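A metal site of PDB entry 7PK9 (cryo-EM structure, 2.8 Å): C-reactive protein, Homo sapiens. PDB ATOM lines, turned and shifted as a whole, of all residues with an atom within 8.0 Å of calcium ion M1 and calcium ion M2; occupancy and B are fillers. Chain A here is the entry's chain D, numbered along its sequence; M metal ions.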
ATOM      1  N   SER A  50     -13.942  28.845 -23.844  1.00  0.00           N
ATOM      2  CA  SER A  50     -15.176  28.970 -23.067  1.00  0.00           C
ATOM      3  C   SER A  50     -16.172  29.947 -23.657  1.00  0.00           C
ATOM      4  O   SER A  50     -15.897  31.140 -23.764  1.00  0.00           O
ATOM      5  CB  SER A  50     -14.837  29.407 -21.637  1.00  0.00           C
ATOM      6  OG  SER A  50     -16.031  29.593 -20.907  1.00  0.00           O
ATOM      7  N   SER A  53     -19.790  30.520 -18.838  1.00  0.00           N
ATOM      8  CA  SER A  53     -19.132  30.019 -17.634  1.00  0.00           C
ATOM      9  C   SER A  53     -19.901  30.532 -16.424  1.00  0.00           C
ATOM     10  O   SER A  53     -19.871  31.718 -16.117  1.00  0.00           O
ATOM     11  CB  SER A  53     -17.678  30.456 -17.580  1.00  0.00           C
ATOM     12  OG  SER A  53     -17.150  30.228 -16.292  1.00  0.00           O
ATOM     13  N   TYR A  54     -20.589  29.604 -15.772  1.00  0.00           N
ATOM     14  CA  TYR A  54     -21.411  29.830 -14.586  1.00  0.00           C
ATOM     15  C   TYR A  54     -20.711  29.180 -13.406  1.00  0.00           C
ATOM     16  O   TYR A  54     -20.683  27.946 -13.299  1.00  0.00           O
ATOM     17  CB  TYR A  54     -22.785  29.235 -14.835  1.00  0.00           C
ATOM     18  CG  TYR A  54     -23.890  29.597 -13.880  1.00  0.00           C
ATOM     19  CD1 TYR A  54     -23.817  29.252 -12.541  1.00  0.00           C
ATOM     20  CD2 TYR A  54     -25.013  30.264 -14.317  1.00  0.00           C
ATOM     21  CE1 TYR A  54     -24.830  29.570 -11.674  1.00  0.00           C
ATOM     22  CE2 TYR A  54     -26.028  30.575 -13.463  1.00  0.00           C
ATOM     23  CZ  TYR A  54     -25.935  30.216 -12.143  1.00  0.00           C
ATOM     24  OH  TYR A  54     -26.961  30.531 -11.298  1.00  0.00           O
ATOM     25  N   ALA A  55     -20.160  29.988 -12.506  1.00  0.00           N
ATOM     26  CA  ALA A  55     -19.521  29.463 -11.310  1.00  0.00           C
ATOM     27  C   ALA A  55     -20.329  29.788 -10.074  1.00  0.00           C
ATOM     28  O   ALA A  55     -21.052  30.782 -10.011  1.00  0.00           O
ATOM     29  CB  ALA A  55     -18.114  30.041 -11.146  1.00  0.00           C
ATOM     30  N   GLN A  59     -18.687  25.297  -6.718  1.00  0.00           N
ATOM     31  CA  GLN A  59     -18.416  24.585  -7.965  1.00  0.00           C
ATOM     32  C   GLN A  59     -18.084  25.617  -9.031  1.00  0.00           C
ATOM     33  O   GLN A  59     -18.946  26.434  -9.377  1.00  0.00           O
ATOM     34  CB  GLN A  59     -19.626  23.744  -8.366  1.00  0.00           C
ATOM     35  CG  GLN A  59     -19.520  23.007  -9.687  1.00  0.00           C
ATOM     36  CD  GLN A  59     -18.339  22.075  -9.748  1.00  0.00           C
ATOM     37  OE1 GLN A  59     -17.293  22.405 -10.311  1.00  0.00           O
ATOM     38  NE2 GLN A  59     -18.484  20.891  -9.164  1.00  0.00           N
ATOM     39  N   ASP A  60     -16.849  25.607  -9.521  1.00  0.00           N
ATOM     40  CA  ASP A  60     -16.435  26.559 -10.548  1.00  0.00           C
ATOM     41  C   ASP A  60     -17.124  26.320 -11.885  1.00  0.00           C
ATOM     42  O   ASP A  60     -17.222  27.254 -12.687  1.00  0.00           O
ATOM     43  CB  ASP A  60     -14.921  26.518 -10.733  1.00  0.00           C
ATOM     44  CG  ASP A  60     -14.446  25.213 -11.352  1.00  0.00           C
ATOM     45  OD1 ASP A  60     -15.294  24.415 -11.766  1.00  0.00           O
ATOM     46  OD2 ASP A  60     -13.222  25.005 -11.444  1.00  0.00           O
ATOM     47  N   ASN A  61     -17.571  25.095 -12.156  1.00  0.00           N
ATOM     48  CA  ASN A  61     -18.125  24.720 -13.441  1.00  0.00           C
ATOM     49  C   ASN A  61     -19.576  24.309 -13.298  1.00  0.00           C
ATOM     50  O   ASN A  61     -19.930  23.172 -13.647  1.00  0.00           O
ATOM     51  CB  ASN A  61     -17.326  23.598 -14.095  1.00  0.00           C
ATOM     52  CG  ASN A  61     -15.906  23.976 -14.352  1.00  0.00           C
ATOM     53  OD1 ASN A  61     -15.537  25.141 -14.248  1.00  0.00           O
ATOM     54  ND2 ASN A  61     -15.091  23.001 -14.715  1.00  0.00           N
ATOM     55  N   GLU A  62     -20.409  25.191 -12.778  1.00  0.00           N
ATOM     56  CA  GLU A  62     -21.795  24.823 -12.523  1.00  0.00           C
ATOM     57  C   GLU A  62     -22.583  24.728 -13.825  1.00  0.00           C
ATOM     58  O   GLU A  62     -23.390  23.815 -13.998  1.00  0.00           O
ATOM     59  CB  GLU A  62     -22.424  25.838 -11.587  1.00  0.00           C
ATOM     60  CG  GLU A  62     -23.817  25.499 -11.120  1.00  0.00           C
ATOM     61  CD  GLU A  62     -23.802  24.646  -9.871  1.00  0.00           C
ATOM     62  OE1 GLU A  62     -24.872  24.487  -9.250  1.00  0.00           O
ATOM     63  OE2 GLU A  62     -22.728  24.116  -9.525  1.00  0.00           O
ATOM     64  N   ILE A  63     -22.366  25.662 -14.740  1.00  0.00           N
ATOM     65  CA  ILE A  63     -22.626  25.445 -16.162  1.00  0.00           C
ATOM     66  C   ILE A  63     -21.394  25.880 -16.915  1.00  0.00           C
ATOM     67  O   ILE A  63     -20.892  26.991 -16.705  1.00  0.00           O
ATOM     68  CB  ILE A  63     -23.856  26.223 -16.651  1.00  0.00           C
ATOM     69  CG1 ILE A  63     -25.041  26.000 -15.711  1.00  0.00           C
ATOM     70  CG2 ILE A  63     -24.230  25.812 -18.049  1.00  0.00           C
ATOM     71  CD1 ILE A  63     -26.152  26.995 -15.913  1.00  0.00           C
ATOM     72  N   LEU A  64     -20.905  25.030 -17.813  1.00  0.00           N
ATOM     73  CA  LEU A  64     -19.890  25.399 -18.782  1.00  0.00           C
ATOM     74  C   LEU A  64     -20.397  25.010 -20.155  1.00  0.00           C
ATOM     75  O   LEU A  64     -20.777  23.858 -20.370  1.00  0.00           O
ATOM     76  CB  LEU A  64     -18.563  24.711 -18.469  1.00  0.00           C
ATOM     77  CG  LEU A  64     -17.346  25.189 -19.243  1.00  0.00           C
ATOM     78  CD1 LEU A  64     -17.056  26.638 -18.996  1.00  0.00           C
ATOM     79  CD2 LEU A  64     -16.141  24.346 -18.870  1.00  0.00           C
ATOM     80  N   PHE A  66     -18.463  24.774 -23.392  1.00  0.00           N
ATOM     81  CA  PHE A  66     -17.063  24.774 -23.792  1.00  0.00           C
ATOM     82  C   PHE A  66     -16.899  24.084 -25.131  1.00  0.00           C
ATOM     83  O   PHE A  66     -17.247  22.906 -25.280  1.00  0.00           O
ATOM     84  CB  PHE A  66     -16.216  24.062 -22.730  1.00  0.00           C
ATOM     85  CG  PHE A  66     -14.766  24.420 -22.787  1.00  0.00           C
ATOM     86  CD1 PHE A  66     -14.260  25.446 -22.030  1.00  0.00           C
ATOM     87  CD2 PHE A  66     -13.910  23.676 -23.571  1.00  0.00           C
ATOM     88  CE1 PHE A  66     -12.936  25.757 -22.091  1.00  0.00           C
ATOM     89  CE2 PHE A  66     -12.586  23.987 -23.632  1.00  0.00           C
ATOM     90  CZ  PHE A  66     -12.094  25.025 -22.888  1.00  0.00           C
ATOM     91  N   THR A  76     -21.437  20.987 -19.677  1.00  0.00           N
ATOM     92  CA  THR A  76     -21.276  20.412 -18.349  1.00  0.00           C
ATOM     93  C   THR A  76     -22.234  21.067 -17.380  1.00  0.00           C
ATOM     94  O   THR A  76     -22.472  22.275 -17.457  1.00  0.00           O
ATOM     95  CB  THR A  76     -19.869  20.602 -17.800  1.00  0.00           C
ATOM     96  OG1 THR A  76     -19.651  21.995 -17.568  1.00  0.00           O
ATOM     97  CG2 THR A  76     -18.838  20.162 -18.789  1.00  0.00           C
ATOM     98  N   GLN A 137     -14.010  34.361 -20.477  1.00  0.00           N
ATOM     99  CA  GLN A 137     -13.031  33.581 -19.730  1.00  0.00           C
ATOM    100  C   GLN A 137     -13.703  32.350 -19.162  1.00  0.00           C
ATOM    101  O   GLN A 137     -14.910  32.311 -18.965  1.00  0.00           O
ATOM    102  CB  GLN A 137     -12.388  34.391 -18.603  1.00  0.00           C
ATOM    103  CG  GLN A 137     -11.649  35.635 -19.026  1.00  0.00           C
ATOM    104  CD  GLN A 137     -10.487  35.320 -19.925  1.00  0.00           C
ATOM    105  OE1 GLN A 137      -9.956  34.217 -19.901  1.00  0.00           O
ATOM    106  NE2 GLN A 137     -10.045  36.303 -20.690  1.00  0.00           N
ATOM    107  N   GLU A 138     -12.884  31.347 -18.879  1.00  0.00           N
ATOM    108  CA  GLU A 138     -13.276  30.168 -18.122  1.00  0.00           C
ATOM    109  C   GLU A 138     -12.775  30.342 -16.705  1.00  0.00           C
ATOM    110  O   GLU A 138     -11.564  30.358 -16.469  1.00  0.00           O
ATOM    111  CB  GLU A 138     -12.704  28.914 -18.783  1.00  0.00           C
ATOM    112  CG  GLU A 138     -13.548  27.680 -18.649  1.00  0.00           C
ATOM    113  CD  GLU A 138     -13.568  27.134 -17.244  1.00  0.00           C
ATOM    114  OE1 GLU A 138     -12.483  26.985 -16.650  1.00  0.00           O
ATOM    115  OE2 GLU A 138     -14.671  26.831 -16.727  1.00  0.00           O
ATOM    116  N   GLN A 139     -13.689  30.454 -15.759  1.00  0.00           N
ATOM    117  CA  GLN A 139     -13.318  30.672 -14.371  1.00  0.00           C
ATOM    118  C   GLN A 139     -13.129  29.330 -13.688  1.00  0.00           C
ATOM    119  O   GLN A 139     -13.954  28.423 -13.836  1.00  0.00           O
ATOM    120  CB  GLN A 139     -14.336  31.531 -13.639  1.00  0.00           C
ATOM    121  CG  GLN A 139     -15.672  30.908 -13.393  1.00  0.00           C
ATOM    122  CD  GLN A 139     -16.732  31.976 -13.213  1.00  0.00           C
ATOM    123  OE1 GLN A 139     -16.481  33.008 -12.614  1.00  0.00           O
ATOM    124  NE2 GLN A 139     -17.928  31.713 -13.707  1.00  0.00           N
ATOM    125  N   ASP A 140     -12.038  29.213 -12.933  1.00  0.00           N
ATOM    126  CA  ASP A 140     -11.740  28.063 -12.103  1.00  0.00           C
ATOM    127  C   ASP A 140     -11.936  28.342 -10.620  1.00  0.00           C
ATOM    128  O   ASP A 140     -11.598  27.492  -9.803  1.00  0.00           O
ATOM    129  CB  ASP A 140     -10.306  27.594 -12.362  1.00  0.00           C
ATOM    130  CG  ASP A 140     -10.100  27.093 -13.777  1.00  0.00           C
ATOM    131  OD1 ASP A 140      -9.840  27.924 -14.674  1.00  0.00           O
ATOM    132  OD2 ASP A 140     -10.211  25.874 -13.996  1.00  0.00           O
ATOM    133  N   SER A 141     -12.455  29.510 -10.277  1.00  0.00           N
ATOM    134  CA  SER A 141     -12.959  29.753  -8.930  1.00  0.00           C
ATOM    135  C   SER A 141     -14.253  30.533  -9.077  1.00  0.00           C
ATOM    136  O   SER A 141     -14.824  30.630 -10.167  1.00  0.00           O
ATOM    137  CB  SER A 141     -11.923  30.496  -8.069  1.00  0.00           C
ATOM    138  OG  SER A 141     -11.653  31.786  -8.576  1.00  0.00           O
ATOM    139  N   GLY A 144     -12.339  33.921 -10.975  1.00  0.00           N
ATOM    140  CA  GLY A 144     -10.973  34.185 -11.358  1.00  0.00           C
ATOM    141  C   GLY A 144     -10.235  32.938 -11.790  1.00  0.00           C
ATOM    142  O   GLY A 144     -10.842  31.932 -12.161  1.00  0.00           O
ATOM    143  N   ASN A 145      -8.916  33.025 -11.730  1.00  0.00           N
ATOM    144  CA  ASN A 145      -8.040  31.964 -12.217  1.00  0.00           C
ATOM    145  C   ASN A 145      -8.263  31.705 -13.704  1.00  0.00           C
ATOM    146  O   ASN A 145      -8.299  30.561 -14.162  1.00  0.00           O
ATOM    147  CB  ASN A 145      -8.212  30.680 -11.406  1.00  0.00           C
ATOM    148  CG  ASN A 145      -8.038  30.903  -9.933  1.00  0.00           C
ATOM    149  OD1 ASN A 145      -7.135  31.631  -9.514  1.00  0.00           O
ATOM    150  ND2 ASN A 145      -8.881  30.270  -9.133  1.00  0.00           N
ATOM    151  N   PHE A 146      -8.441  32.784 -14.458  1.00  0.00           N
ATOM    152  CA  PHE A 146      -8.616  32.672 -15.893  1.00  0.00           C
ATOM    153  C   PHE A 146      -7.382  32.083 -16.567  1.00  0.00           C
ATOM    154  O   PHE A 146      -6.261  32.214 -16.072  1.00  0.00           O
ATOM    155  CB  PHE A 146      -8.985  34.029 -16.483  1.00  0.00           C
ATOM    156  CG  PHE A 146     -10.081  34.727 -15.735  1.00  0.00           C
ATOM    157  CD1 PHE A 146     -11.256  34.064 -15.451  1.00  0.00           C
ATOM    158  CD2 PHE A 146      -9.931  36.027 -15.305  1.00  0.00           C
ATOM    159  CE1 PHE A 146     -12.267  34.682 -14.762  1.00  0.00           C
ATOM    160  CE2 PHE A 146     -10.946  36.654 -14.620  1.00  0.00           C
ATOM    161  CZ  PHE A 146     -12.113  35.974 -14.353  1.00  0.00           C
ATOM    162  N   GLU A 147      -7.609  31.425 -17.694  1.00  0.00           N
ATOM    163  CA  GLU A 147      -6.570  30.807 -18.500  1.00  0.00           C
ATOM    164  C   GLU A 147      -6.676  31.373 -19.913  1.00  0.00           C
ATOM    165  O   GLU A 147      -7.747  31.309 -20.525  1.00  0.00           O
ATOM    166  CB  GLU A 147      -6.707  29.287 -18.523  1.00  0.00           C
ATOM    167  CG  GLU A 147      -6.755  28.639 -17.164  1.00  0.00           C
ATOM    168  CD  GLU A 147      -7.300  27.226 -17.214  1.00  0.00           C
ATOM    169  OE1 GLU A 147      -8.493  27.039 -16.899  1.00  0.00           O
ATOM    170  OE2 GLU A 147      -6.534  26.304 -17.573  1.00  0.00           O
ATOM    171  N   SER A 149      -5.301  30.303 -22.763  1.00  0.00           N
ATOM    172  CA  SER A 149      -5.643  29.194 -23.646  1.00  0.00           C
ATOM    173  C   SER A 149      -7.129  28.812 -23.660  1.00  0.00           C
ATOM    174  O   SER A 149      -7.538  28.031 -24.514  1.00  0.00           O
ATOM    175  CB  SER A 149      -4.829  27.967 -23.242  1.00  0.00           C
ATOM    176  OG  SER A 149      -5.117  27.579 -21.914  1.00  0.00           O
ATOM    177  N   GLN A 150      -7.927  29.340 -22.736  1.00  0.00           N
ATOM    178  CA  GLN A 150      -9.357  29.073 -22.723  1.00  0.00           C
ATOM    179  C   GLN A 150     -10.212  30.297 -23.030  1.00  0.00           C
ATOM    180  O   GLN A 150     -11.420  30.146 -23.234  1.00  0.00           O
ATOM    181  CB  GLN A 150      -9.769  28.465 -21.371  1.00  0.00           C
ATOM    182  CG  GLN A 150      -8.962  27.249 -21.012  1.00  0.00           C
ATOM    183  CD  GLN A 150      -9.576  26.452 -19.900  1.00  0.00           C
ATOM    184  OE1 GLN A 150     -10.284  26.989 -19.052  1.00  0.00           O
ATOM    185  NE2 GLN A 150      -9.343  25.151 -19.894  1.00  0.00           N
HETATM  186 CA    CA M   1     -10.361  26.133 -16.258  1.00  0.00          CA
HETATM  187 CA    CA M   2     -13.427  25.728 -14.909  1.00  0.00          CA
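Merely in contact with calcium ion M2: Asp 60 (3.5 Å).
Of the 23 residues printed, 5 come within 4 Å of calcium ion M2.
The backbone NH (N) of Ser 50 lies within hydrogen-bond range of the backbone carbonyl oxygen (O) of Gln 150 (2.9 Å).
OE1 of Gln 150 sits close to OE1 of Glu 147, at 2.8 Å.
The backbone NH (N) of Asn 61 lies close to the side-chain amide oxygen (OE1) of Gln 59, 3.3 Å away.
The side-chain amide nitrogen (NE2) of Gln 139 lies within hydrogen-bond range of the side-chain hydroxyl (OG) of Ser 53 (3.1 Å).
The side-chain amide nitrogen of Asn 61 lies close to the side-chain carboxylate of Asp 60, at 3.3 Å.
The side-chain amide nitrogen of Gln 139 sits close to the backbone NH of Ala 55, at 3.1 Å.
The side-chain carboxylate of Asp 60 sits close to the side-chain amide oxygen of Gln 59.
OE1 of Gln 150 sits close to OE1 of Glu 138.
The side-chain amide oxygen (OD1) of Asn 61 is bound to calcium ion M2, 2.3 Å away.
Calcium ion M2 is bound by OE1 of Glu 138, at 2.3 Å.
Calcium ion M2 is bound by OE2 of Glu 138 (2.5 Å).
Slightly farther from calcium ion M2 lies O of Gln 139 (2.9 Å).
Calcium ion M1 is bound by the side-chain carboxylate (OE1) of Glu 147, the side-chain carboxylate (OD2) of Asp 140, the side-chain carboxylate (OE1) of Glu 138 and the side-chain carboxylate (OD1) of Asp 140.
Slightly farther from calcium ion M1 lies OE1 of Gln 150 (2.9 Å).
Within 4 Å of calcium ion M1: Glu 138, Asp 140, Glu 147 and Gln 150.
The nearest printed residue that does not touch calcium ion M1 is Gln 139 (4.9 Å).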
